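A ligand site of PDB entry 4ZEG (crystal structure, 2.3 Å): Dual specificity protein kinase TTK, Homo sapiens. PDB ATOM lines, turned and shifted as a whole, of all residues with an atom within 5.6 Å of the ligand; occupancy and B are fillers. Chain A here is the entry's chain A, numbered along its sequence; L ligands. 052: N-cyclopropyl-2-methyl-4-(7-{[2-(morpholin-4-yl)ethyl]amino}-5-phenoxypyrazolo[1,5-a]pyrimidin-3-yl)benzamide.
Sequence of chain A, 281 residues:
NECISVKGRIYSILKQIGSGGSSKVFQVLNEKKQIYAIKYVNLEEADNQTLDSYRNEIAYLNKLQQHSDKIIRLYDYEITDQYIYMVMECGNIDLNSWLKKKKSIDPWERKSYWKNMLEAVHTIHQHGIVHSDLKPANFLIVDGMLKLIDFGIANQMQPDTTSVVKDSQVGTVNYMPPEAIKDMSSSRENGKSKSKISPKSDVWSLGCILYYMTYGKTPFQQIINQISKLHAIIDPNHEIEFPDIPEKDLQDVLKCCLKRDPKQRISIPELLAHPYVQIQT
The backbone NH (N) of Gly 91 lies within hydrogen-bond range of a nitrogen (N5) of the ligand, 3.0 Å away. NZ of Lys 39 is in hydrogen-bond range of O3 of the ligand (3.0 Å). A nitrogen (N2) of the ligand sits at hydrogen-bond distance from the backbone carbonyl oxygen (O) of Gly 91, at 3.1 Å. A nitrogen (N6) of the ligand sits at hydrogen-bond distance from the backbone carbonyl oxygen (O) of Ile 149, at 2.8 Å.
Merely in contact with the ligand: Ala 137, Asn 92, Glu 89, Leu 140, Glu 57, Ala 37, Ile 17, Gln 158, Cys 90, Met 157, Val 25, Met 88, Met 86, Pro 159, Asp 150, Lys 15 and Asp 94. Hydrophobic or aromatic side chains within 4 Å of the ligand: Ile 17, Val 25, Ala 37, Met 86, Met 88, Leu 140, Ile 149 and Met 157. Within 4 Å of the ligand: Lys 15, Ile 17, Val 25, Ala 37, Lys 39, Glu 57, Met 86, Met 88, Glu 89, Cys 90, Gly 91, Asn 92, Asp 94, Ala 137, Leu 140, Ile 149, Asp 150, Met 157, Gln 158 and Pro 159. The nearest printed residue that does not touch the ligand is Leu 61 (4.02 Å).
The backbone carbonyl oxygen of Asn 138 sits at hydrogen-bond distance from the backbone NH of Ile 149, 2.9 Å away. The backbone NH of Gln 158 sits at hydrogen-bond distance from the backbone carbonyl oxygen of Ser 19. The side-chain amino group (NZ) of Lys 39 lies within salt-bridge range of the side-chain carboxylate (OE1) of Glu 57, 2.9 Å away. N of Ala 37 is in hydrogen-bond range of O of Met 88 (2.7 Å). OD1 of Asp 150 is in hydrogen-bond range of ND2 of Asn 138 (2.9 Å). The backbone NH (N) of Ile 17 sits at hydrogen-bond distance from the backbone carbonyl oxygen (O) of Val 25 (2.8 Å). The backbone NH (N) of Val 25 is in hydrogen-bond range of the backbone carbonyl oxygen (O) of Gly 18. O of Lys 39 is in hydrogen-bond range of N of Met 86 (2.8 Å).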
ATOM      1  N   LYS A  15      11.637   4.484 -13.023  1.00  0.00           N
ATOM      2  CA  LYS A  15      12.070   5.352 -14.074  1.00  0.00           C
ATOM      3  C   LYS A  15      11.446   6.721 -13.909  1.00  0.00           C
ATOM      4  O   LYS A  15      10.611   6.945 -13.040  1.00  0.00           O
ATOM      5  CB  LYS A  15      11.742   4.758 -15.438  1.00  0.00           C
ATOM      6  CG  LYS A  15      10.279   4.400 -15.631  1.00  0.00           C
ATOM      7  CD  LYS A  15       9.972   4.043 -17.074  1.00  0.00           C
ATOM      8  CE  LYS A  15      10.433   5.113 -18.059  1.00  0.00           C
ATOM      9  NZ  LYS A  15      10.025   4.812 -19.471  1.00  0.00           N
ATOM     10  N   ILE A  17       9.314   9.515 -15.510  1.00  0.00           N
ATOM     11  CA  ILE A  17       8.239   9.551 -16.493  1.00  0.00           C
ATOM     12  C   ILE A  17       7.949  10.957 -16.925  1.00  0.00           C
ATOM     13  O   ILE A  17       7.128  11.175 -17.797  1.00  0.00           O
ATOM     14  CB  ILE A  17       6.952   8.883 -15.983  1.00  0.00           C
ATOM     15  CG1 ILE A  17       6.437   9.579 -14.707  1.00  0.00           C
ATOM     16  CG2 ILE A  17       7.199   7.395 -15.756  1.00  0.00           C
ATOM     17  CD1 ILE A  17       5.303   8.794 -14.035  1.00  0.00           C
ATOM     18  N   GLY A  18       8.607  11.921 -16.307  1.00  0.00           N
ATOM     19  CA  GLY A  18       8.312  13.292 -16.649  1.00  0.00           C
ATOM     20  C   GLY A  18       9.281  14.293 -16.096  1.00  0.00           C
ATOM     21  O   GLY A  18       9.987  14.038 -15.143  1.00  0.00           O
ATOM     22  N   SER A  19       9.266  15.474 -16.664  1.00  0.00           N
ATOM     23  CA  SER A  19      10.282  16.436 -16.362  1.00  0.00           C
ATOM     24  C   SER A  19       9.764  17.826 -16.620  1.00  0.00           C
ATOM     25  O   SER A  19       8.855  18.037 -17.432  1.00  0.00           O
ATOM     26  CB  SER A  19      11.468  16.166 -17.261  1.00  0.00           C
ATOM     27  OG  SER A  19      12.572  16.831 -16.732  1.00  0.00           O
ATOM     28  N   VAL A  25       9.227  13.898 -12.368  1.00  0.00           N
ATOM     29  CA  VAL A  25       8.264  12.898 -11.915  1.00  0.00           C
ATOM     30  C   VAL A  25       8.817  11.486 -12.156  1.00  0.00           C
ATOM     31  O   VAL A  25       9.244  11.169 -13.239  1.00  0.00           O
ATOM     32  CB  VAL A  25       6.900  13.046 -12.625  1.00  0.00           C
ATOM     33  CG1 VAL A  25       5.822  12.211 -11.943  1.00  0.00           C
ATOM     34  CG2 VAL A  25       6.478  14.481 -12.594  1.00  0.00           C
ATOM     35  N   GLN A  27       8.231   7.266 -11.693  1.00  0.00           N
ATOM     36  CA  GLN A  27       7.482   6.060 -11.339  1.00  0.00           C
ATOM     37  C   GLN A  27       8.281   5.302 -10.327  1.00  0.00           C
ATOM     38  O   GLN A  27       9.448   5.172 -10.488  1.00  0.00           O
ATOM     39  CB  GLN A  27       7.288   5.254 -12.599  1.00  0.00           C
ATOM     40  CG  GLN A  27       6.398   4.044 -12.494  1.00  0.00           C
ATOM     41  CD  GLN A  27       6.341   3.309 -13.835  1.00  0.00           C
ATOM     42  OE1 GLN A  27       7.295   3.322 -14.603  1.00  0.00           O
ATOM     43  NE2 GLN A  27       5.228   2.692 -14.115  1.00  0.00           N
ATOM     44  N   ALA A  37       3.480   7.526  -8.347  1.00  0.00           N
ATOM     45  CA  ALA A  37       4.215   8.555  -9.057  1.00  0.00           C
ATOM     46  C   ALA A  37       4.697   9.538  -8.000  1.00  0.00           C
ATOM     47  O   ALA A  37       3.921   9.955  -7.159  1.00  0.00           O
ATOM     48  CB  ALA A  37       3.339   9.251 -10.083  1.00  0.00           C
ATOM     49  N   LYS A  39       6.435  13.222  -7.534  1.00  0.00           N
ATOM     50  CA  LYS A  39       6.999  14.472  -8.069  1.00  0.00           C
ATOM     51  C   LYS A  39       8.040  14.999  -7.080  1.00  0.00           C
ATOM     52  O   LYS A  39       7.753  15.084  -5.871  1.00  0.00           O
ATOM     53  CB  LYS A  39       5.946  15.580  -8.275  1.00  0.00           C
ATOM     54  CG  LYS A  39       6.627  16.829  -8.847  1.00  0.00           C
ATOM     55  CD  LYS A  39       5.729  17.692  -9.727  1.00  0.00           C
ATOM     56  CE  LYS A  39       4.775  18.517  -8.906  1.00  0.00           C
ATOM     57  NZ  LYS A  39       3.903  19.318  -9.820  1.00  0.00           N
ATOM     58  N   GLU A  57      -0.662  24.674  -5.477  1.00  0.00           N
ATOM     59  CA  GLU A  57      -0.984  23.317  -6.051  1.00  0.00           C
ATOM     60  C   GLU A  57      -1.225  22.259  -5.035  1.00  0.00           C
ATOM     61  O   GLU A  57      -2.210  21.539  -5.090  1.00  0.00           O
ATOM     62  CB  GLU A  57       0.178  22.858  -6.916  1.00  0.00           C
ATOM     63  CG  GLU A  57      -0.094  21.742  -7.905  1.00  0.00           C
ATOM     64  CD  GLU A  57       1.130  21.497  -8.741  1.00  0.00           C
ATOM     65  OE1 GLU A  57       2.139  20.990  -8.178  1.00  0.00           O
ATOM     66  OE2 GLU A  57       1.110  21.873  -9.931  1.00  0.00           O
ATOM     67  N   LEU A  61      -4.662  20.401  -4.560  1.00  0.00           N
ATOM     68  CA  LEU A  61      -4.677  18.988  -4.766  1.00  0.00           C
ATOM     69  C   LEU A  61      -5.222  18.291  -3.531  1.00  0.00           C
ATOM     70  O   LEU A  61      -6.080  17.392  -3.612  1.00  0.00           O
ATOM     71  CB  LEU A  61      -3.270  18.448  -5.113  1.00  0.00           C
ATOM     72  CG  LEU A  61      -3.225  16.965  -5.433  1.00  0.00           C
ATOM     73  CD1 LEU A  61      -4.222  16.573  -6.503  1.00  0.00           C
ATOM     74  CD2 LEU A  61      -1.821  16.471  -5.789  1.00  0.00           C
ATOM     75  N   ILE A  72      -6.309  13.181  -9.817  1.00  0.00           N
ATOM     76  CA  ILE A  72      -5.203  12.392  -9.335  1.00  0.00           C
ATOM     77  C   ILE A  72      -5.157  12.383  -7.807  1.00  0.00           C
ATOM     78  O   ILE A  72      -5.425  13.391  -7.151  1.00  0.00           O
ATOM     79  CB  ILE A  72      -3.886  12.887 -10.001  1.00  0.00           C
ATOM     80  CG1 ILE A  72      -2.777  11.851  -9.869  1.00  0.00           C
ATOM     81  CG2 ILE A  72      -3.417  14.200  -9.440  1.00  0.00           C
ATOM     82  CD1 ILE A  72      -2.937  10.728 -10.865  1.00  0.00           C
ATOM     83  N   MET A  86       6.003  14.825  -3.695  1.00  0.00           N
ATOM     84  CA  MET A  86       4.627  14.458  -3.684  1.00  0.00           C
ATOM     85  C   MET A  86       4.464  12.992  -4.149  1.00  0.00           C
ATOM     86  O   MET A  86       4.821  12.639  -5.257  1.00  0.00           O
ATOM     87  CB  MET A  86       3.860  15.419  -4.615  1.00  0.00           C
ATOM     88  CG  MET A  86       3.864  16.890  -4.146  1.00  0.00           C
ATOM     89  SD  MET A  86       3.324  18.147  -5.313  1.00  0.00           S
ATOM     90  CE  MET A  86       1.582  17.814  -5.224  1.00  0.00           C
ATOM     91  N   MET A  88       1.888  10.445  -5.410  1.00  0.00           N
ATOM     92  CA  MET A  88       0.586  10.412  -6.027  1.00  0.00           C
ATOM     93  C   MET A  88       0.335   9.116  -6.826  1.00  0.00           C
ATOM     94  O   MET A  88       1.240   8.365  -7.090  1.00  0.00           O
ATOM     95  CB  MET A  88       0.515  11.568  -6.974  1.00  0.00           C
ATOM     96  CG  MET A  88       0.552  12.914  -6.239  1.00  0.00           C
ATOM     97  SD  MET A  88       0.884  14.199  -7.432  1.00  0.00           S
ATOM     98  CE  MET A  88       2.600  13.970  -7.839  1.00  0.00           C
ATOM     99  N   GLU A  89      -0.881   8.892  -7.246  1.00  0.00           N
ATOM    100  CA  GLU A  89      -1.154   7.666  -7.947  1.00  0.00           C
ATOM    101  C   GLU A  89      -0.445   7.707  -9.275  1.00  0.00           C
ATOM    102  O   GLU A  89      -0.144   8.789  -9.781  1.00  0.00           O
ATOM    103  CB  GLU A  89      -2.665   7.363  -8.049  1.00  0.00           C
ATOM    104  CG  GLU A  89      -3.426   7.993  -9.161  1.00  0.00           C
ATOM    105  CD  GLU A  89      -4.948   7.805  -9.002  1.00  0.00           C
ATOM    106  OE1 GLU A  89      -5.654   8.822  -8.833  1.00  0.00           O
ATOM    107  OE2 GLU A  89      -5.450   6.674  -9.063  1.00  0.00           O
ATOM    108  N   CYS A  90      -0.041   6.515  -9.755  1.00  0.00           N
ATOM    109  CA  CYS A  90       0.573   6.309 -11.057  1.00  0.00           C
ATOM    110  C   CYS A  90      -0.508   5.825 -12.015  1.00  0.00           C
ATOM    111  O   CYS A  90      -1.287   4.945 -11.649  1.00  0.00           O
ATOM    112  CB  CYS A  90       1.645   5.191 -10.987  1.00  0.00           C
ATOM    113  SG  CYS A  90       2.604   5.114 -12.505  1.00  0.00           S
ATOM    114  N   GLY A  91      -0.558   6.359 -13.231  1.00  0.00           N
ATOM    115  CA  GLY A  91      -1.477   5.810 -14.250  1.00  0.00           C
ATOM    116  C   GLY A  91      -0.853   4.862 -15.283  1.00  0.00           C
ATOM    117  O   GLY A  91       0.353   4.563 -15.251  1.00  0.00           O
ATOM    118  N   ASN A  92      -1.662   4.412 -16.245  1.00  0.00           N
ATOM    119  CA  ASN A  92      -1.202   3.442 -17.250  1.00  0.00           C
ATOM    120  C   ASN A  92      -0.463   4.215 -18.324  1.00  0.00           C
ATOM    121  O   ASN A  92       0.682   3.911 -18.679  1.00  0.00           O
ATOM    122  CB  ASN A  92      -2.391   2.679 -17.835  1.00  0.00           C
ATOM    123  CG  ASN A  92      -3.308   2.072 -16.764  1.00  0.00           C
ATOM    124  OD1 ASN A  92      -2.854   1.559 -15.738  1.00  0.00           O
ATOM    125  ND2 ASN A  92      -4.616   2.122 -17.010  1.00  0.00           N
ATOM    126  N   ILE A  93      -1.098   5.277 -18.774  1.00  0.00           N
ATOM    127  CA  ILE A  93      -0.538   6.090 -19.841  1.00  0.00           C
ATOM    128  C   ILE A  93      -1.211   7.481 -19.811  1.00  0.00           C
ATOM    129  O   ILE A  93      -2.369   7.609 -19.375  1.00  0.00           O
ATOM    130  CB  ILE A  93      -0.794   5.398 -21.206  1.00  0.00           C
ATOM    131  CG1 ILE A  93      -0.106   6.185 -22.348  1.00  0.00           C
ATOM    132  CG2 ILE A  93      -2.290   5.279 -21.457  1.00  0.00           C
ATOM    133  CD1 ILE A  93      -0.029   5.453 -23.680  1.00  0.00           C
ATOM    134  N   ASP A  94      -0.487   8.501 -20.269  1.00  0.00           N
ATOM    135  CA  ASP A  94      -1.052   9.824 -20.446  1.00  0.00           C
ATOM    136  C   ASP A  94      -1.752   9.901 -21.745  1.00  0.00           C
ATOM    137  O   ASP A  94      -1.356   9.269 -22.716  1.00  0.00           O
ATOM    138  CB  ASP A  94      -0.009  10.949 -20.376  1.00  0.00           C
ATOM    139  CG  ASP A  94       0.817  11.067 -21.605  1.00  0.00           C
ATOM    140  OD1 ASP A  94       1.757  10.276 -21.738  1.00  0.00           O
ATOM    141  OD2 ASP A  94       0.568  11.956 -22.446  1.00  0.00           O
ATOM    142  N   ALA A 137      -1.884  16.013 -22.496  1.00  0.00           N
ATOM    143  CA  ALA A 137      -0.878  15.695 -21.464  1.00  0.00           C
ATOM    144  C   ALA A 137      -1.417  15.859 -20.033  1.00  0.00           C
ATOM    145  O   ALA A 137      -0.974  15.157 -19.108  1.00  0.00           O
ATOM    146  CB  ALA A 137       0.343  16.578 -21.643  1.00  0.00           C
ATOM    147  N   ASN A 138      -2.356  16.794 -19.847  1.00  0.00           N
ATOM    148  CA  ASN A 138      -2.940  17.011 -18.501  1.00  0.00           C
ATOM    149  C   ASN A 138      -3.854  15.887 -18.035  1.00  0.00           C
ATOM    150  O   ASN A 138      -4.305  15.876 -16.861  1.00  0.00           O
ATOM    151  CB  ASN A 138      -3.674  18.335 -18.467  1.00  0.00           C
ATOM    152  CG  ASN A 138      -2.762  19.511 -18.680  1.00  0.00           C
ATOM    153  OD1 ASN A 138      -3.087  20.460 -19.395  1.00  0.00           O
ATOM    154  ND2 ASN A 138      -1.632  19.482 -18.031  1.00  0.00           N
ATOM    155  N   LEU A 140      -4.801  11.565 -17.696  1.00  0.00           N
ATOM    156  CA  LEU A 140      -4.101  10.331 -17.454  1.00  0.00           C
ATOM    157  C   LEU A 140      -5.100   9.190 -17.367  1.00  0.00           C
ATOM    158  O   LEU A 140      -6.107   9.281 -16.668  1.00  0.00           O
ATOM    159  CB  LEU A 140      -3.381  10.422 -16.129  1.00  0.00           C
ATOM    160  CG  LEU A 140      -2.365   9.387 -15.725  1.00  0.00           C
ATOM    161  CD1 LEU A 140      -1.141   9.412 -16.636  1.00  0.00           C
ATOM    162  CD2 LEU A 140      -1.968   9.690 -14.281  1.00  0.00           C
ATOM    163  N   ILE A 149      -4.572  15.520 -13.957  1.00  0.00           N
ATOM    164  CA  ILE A 149      -3.225  15.439 -13.326  1.00  0.00           C
ATOM    165  C   ILE A 149      -2.861  16.761 -12.637  1.00  0.00           C
ATOM    166  O   ILE A 149      -2.240  16.735 -11.582  1.00  0.00           O
ATOM    167  CB  ILE A 149      -2.147  15.198 -14.409  1.00  0.00           C
ATOM    168  CG1 ILE A 149      -2.041  13.716 -14.745  1.00  0.00           C
ATOM    169  CG2 ILE A 149      -0.774  15.697 -14.067  1.00  0.00           C
ATOM    170  CD1 ILE A 149      -1.601  13.565 -16.174  1.00  0.00           C
ATOM    171  N   ASP A 150      -3.186  17.894 -13.248  1.00  0.00           N
ATOM    172  CA  ASP A 150      -2.919  19.194 -12.629  1.00  0.00           C
ATOM    173  C   ASP A 150      -3.941  20.274 -12.959  1.00  0.00           C
ATOM    174  O   ASP A 150      -4.889  20.060 -13.726  1.00  0.00           O
ATOM    175  CB  ASP A 150      -1.529  19.710 -13.014  1.00  0.00           C
ATOM    176  CG  ASP A 150      -1.455  20.073 -14.468  1.00  0.00           C
ATOM    177  OD1 ASP A 150      -1.962  19.248 -15.195  1.00  0.00           O
ATOM    178  OD2 ASP A 150      -0.950  21.152 -14.873  1.00  0.00           O
ATOM    179  N   PHE A 151      -3.705  21.448 -12.379  1.00  0.00           N
ATOM    180  CA  PHE A 151      -4.661  22.536 -12.332  1.00  0.00           C
ATOM    181  C   PHE A 151      -4.171  23.816 -12.988  1.00  0.00           C
ATOM    182  O   PHE A 151      -4.812  24.851 -12.873  1.00  0.00           O
ATOM    183  CB  PHE A 151      -4.934  22.876 -10.879  1.00  0.00           C
ATOM    184  CG  PHE A 151      -5.202  21.708 -10.036  1.00  0.00           C
ATOM    185  CD1 PHE A 151      -6.124  20.748 -10.419  1.00  0.00           C
ATOM    186  CD2 PHE A 151      -4.509  21.546  -8.841  1.00  0.00           C
ATOM    187  CE1 PHE A 151      -6.386  19.646  -9.630  1.00  0.00           C
ATOM    188  CE2 PHE A 151      -4.760  20.460  -8.041  1.00  0.00           C
ATOM    189  CZ  PHE A 151      -5.703  19.502  -8.434  1.00  0.00           C
ATOM    190  N   MET A 157       4.791  20.256 -16.405  1.00  0.00           N
ATOM    191  CA  MET A 157       5.781  19.221 -16.674  1.00  0.00           C
ATOM    192  C   MET A 157       5.449  18.621 -18.008  1.00  0.00           C
ATOM    193  O   MET A 157       4.339  18.778 -18.469  1.00  0.00           O
ATOM    194  CB  MET A 157       5.695  18.098 -15.652  1.00  0.00           C
ATOM    195  CG  MET A 157       5.679  18.507 -14.187  1.00  0.00           C
ATOM    196  SD  MET A 157       7.348  18.746 -13.546  1.00  0.00           S
ATOM    197  CE  MET A 157       7.914  17.110 -13.191  1.00  0.00           C
ATOM    198  N   GLN A 158       6.398  17.932 -18.629  1.00  0.00           N
ATOM    199  CA  GLN A 158       6.136  17.176 -19.844  1.00  0.00           C
ATOM    200  C   GLN A 158       6.591  15.721 -19.736  1.00  0.00           C
ATOM    201  O   GLN A 158       7.518  15.414 -18.999  1.00  0.00           O
ATOM    202  CB  GLN A 158       6.866  17.783 -21.020  1.00  0.00           C
ATOM    203  CG  GLN A 158       6.101  18.841 -21.773  1.00  0.00           C
ATOM    204  CD  GLN A 158       6.728  19.149 -23.125  1.00  0.00           C
ATOM    205  OE1 GLN A 158       7.408  18.300 -23.715  1.00  0.00           O
ATOM    206  NE2 GLN A 158       6.515  20.363 -23.614  1.00  0.00           N
ATOM    207  N   PRO A 159       5.959  14.835 -20.525  1.00  0.00           N
ATOM    208  CA  PRO A 159       6.306  13.415 -20.435  1.00  0.00           C
ATOM    209  C   PRO A 159       7.707  13.102 -20.912  1.00  0.00           C
ATOM    210  O   PRO A 159       8.107  13.630 -21.930  1.00  0.00           O
ATOM    211  CB  PRO A 159       5.268  12.733 -21.339  1.00  0.00           C
ATOM    212  CG  PRO A 159       4.207  13.766 -21.636  1.00  0.00           C
ATOM    213  CD  PRO A 159       4.786  15.102 -21.389  1.00  0.00           C
ATOM    214  N   ASP A 160       8.467  12.292 -20.152  1.00  0.00           N
ATOM    215  CA  ASP A 160       9.743  11.708 -20.640  1.00  0.00           C
ATOM    216  C   ASP A 160       9.512  10.303 -21.163  1.00  0.00           C
ATOM    217  O   ASP A 160       9.018  10.186 -22.267  1.00  0.00           O
ATOM    218  CB  ASP A 160      10.802  11.651 -19.542  1.00  0.00           C
ATOM    219  CG  ASP A 160      11.166  13.026 -19.023  1.00  0.00           C
ATOM    220  OD1 ASP A 160      10.628  14.045 -19.547  1.00  0.00           O
ATOM    221  OD2 ASP A 160      11.990  13.099 -18.089  1.00  0.00           O
HETATM  222  C11 052 L   1       1.563  10.888 -13.306  1.00  0.00           C
HETATM  223  C13 052 L   1       3.224  15.474 -17.609  1.00  0.00           C
HETATM  224  C14 052 L   1       2.087  14.841 -18.073  1.00  0.00           C
HETATM  225  C16 052 L   1       3.143  12.693 -17.724  1.00  0.00           C
HETATM  226  C17 052 L   1       4.280  13.324 -17.238  1.00  0.00           C
HETATM  227  C18 052 L   1       4.319  14.708 -17.184  1.00  0.00           C
HETATM  228  C19 052 L   1       2.375  14.649 -12.884  1.00  0.00           C
HETATM  229  C21 052 L   1       1.585  12.298 -12.708  1.00  0.00           C
HETATM  230  C22 052 L   1       0.845  12.617 -11.604  1.00  0.00           C
HETATM  231  C23 052 L   1       0.886  13.933 -11.102  1.00  0.00           C
HETATM  232  C24 052 L   1       3.190  15.682 -13.658  1.00  0.00           C
HETATM  233  C25 052 L   1       1.628  14.937 -11.747  1.00  0.00           C
HETATM  234  C26 052 L   1       1.648  16.311 -11.141  1.00  0.00           C
HETATM  235  C28 052 L   1       0.416  18.107  -8.704  1.00  0.00           C
HETATM  236  C29 052 L   1      -0.818  18.509  -9.418  1.00  0.00           C
HETATM  237  C1  052 L   1       5.624   5.372 -18.173  1.00  0.00           C
HETATM  238  C2  052 L   1       6.304   4.428 -19.176  1.00  0.00           C
HETATM  239  O1  052 L   1       5.414   3.431 -19.581  1.00  0.00           O
HETATM  240  C3  052 L   1       4.669   2.787 -18.568  1.00  0.00           C
HETATM  241  C4  052 L   1       3.822   3.800 -17.787  1.00  0.00           C
HETATM  242  N1  052 L   1       4.178   5.198 -18.077  1.00  0.00           N
HETATM  243  C5  052 L   1       3.268   6.353 -17.781  1.00  0.00           C
HETATM  244  C6  052 L   1       2.761   6.184 -16.376  1.00  0.00           C
HETATM  245  N2  052 L   1       1.746   7.164 -16.034  1.00  0.00           N
HETATM  246  N3  052 L   1       2.407  11.313 -15.637  1.00  0.00           N
HETATM  247  C7  052 L   1       2.019   8.578 -15.923  1.00  0.00           C
HETATM  248  C8  052 L   1       2.477   9.299 -16.968  1.00  0.00           C
HETATM  249  C9  052 L   1       2.664  10.647 -16.783  1.00  0.00           C
HETATM  250  C10 052 L   1       1.099   9.730 -12.698  1.00  0.00           C
HETATM  251  C12 052 L   1       1.926  10.557 -14.592  1.00  0.00           C
HETATM  252  N4  052 L   1       1.723   9.244 -14.760  1.00  0.00           N
HETATM  253  N5  052 L   1       1.269   8.697 -13.612  1.00  0.00           N
HETATM  254  O2  052 L   1       3.124  11.302 -17.841  1.00  0.00           O
HETATM  255  C15 052 L   1       2.053  13.447 -18.128  1.00  0.00           C
HETATM  256  C20 052 L   1       2.316  13.329 -13.337  1.00  0.00           C
HETATM  257  O3  052 L   1       2.720  16.813 -10.853  1.00  0.00           O
HETATM  258  N6  052 L   1       0.435  16.984 -10.847  1.00  0.00           N
HETATM  259  C27 052 L   1       0.453  18.261 -10.207  1.00  0.00           C
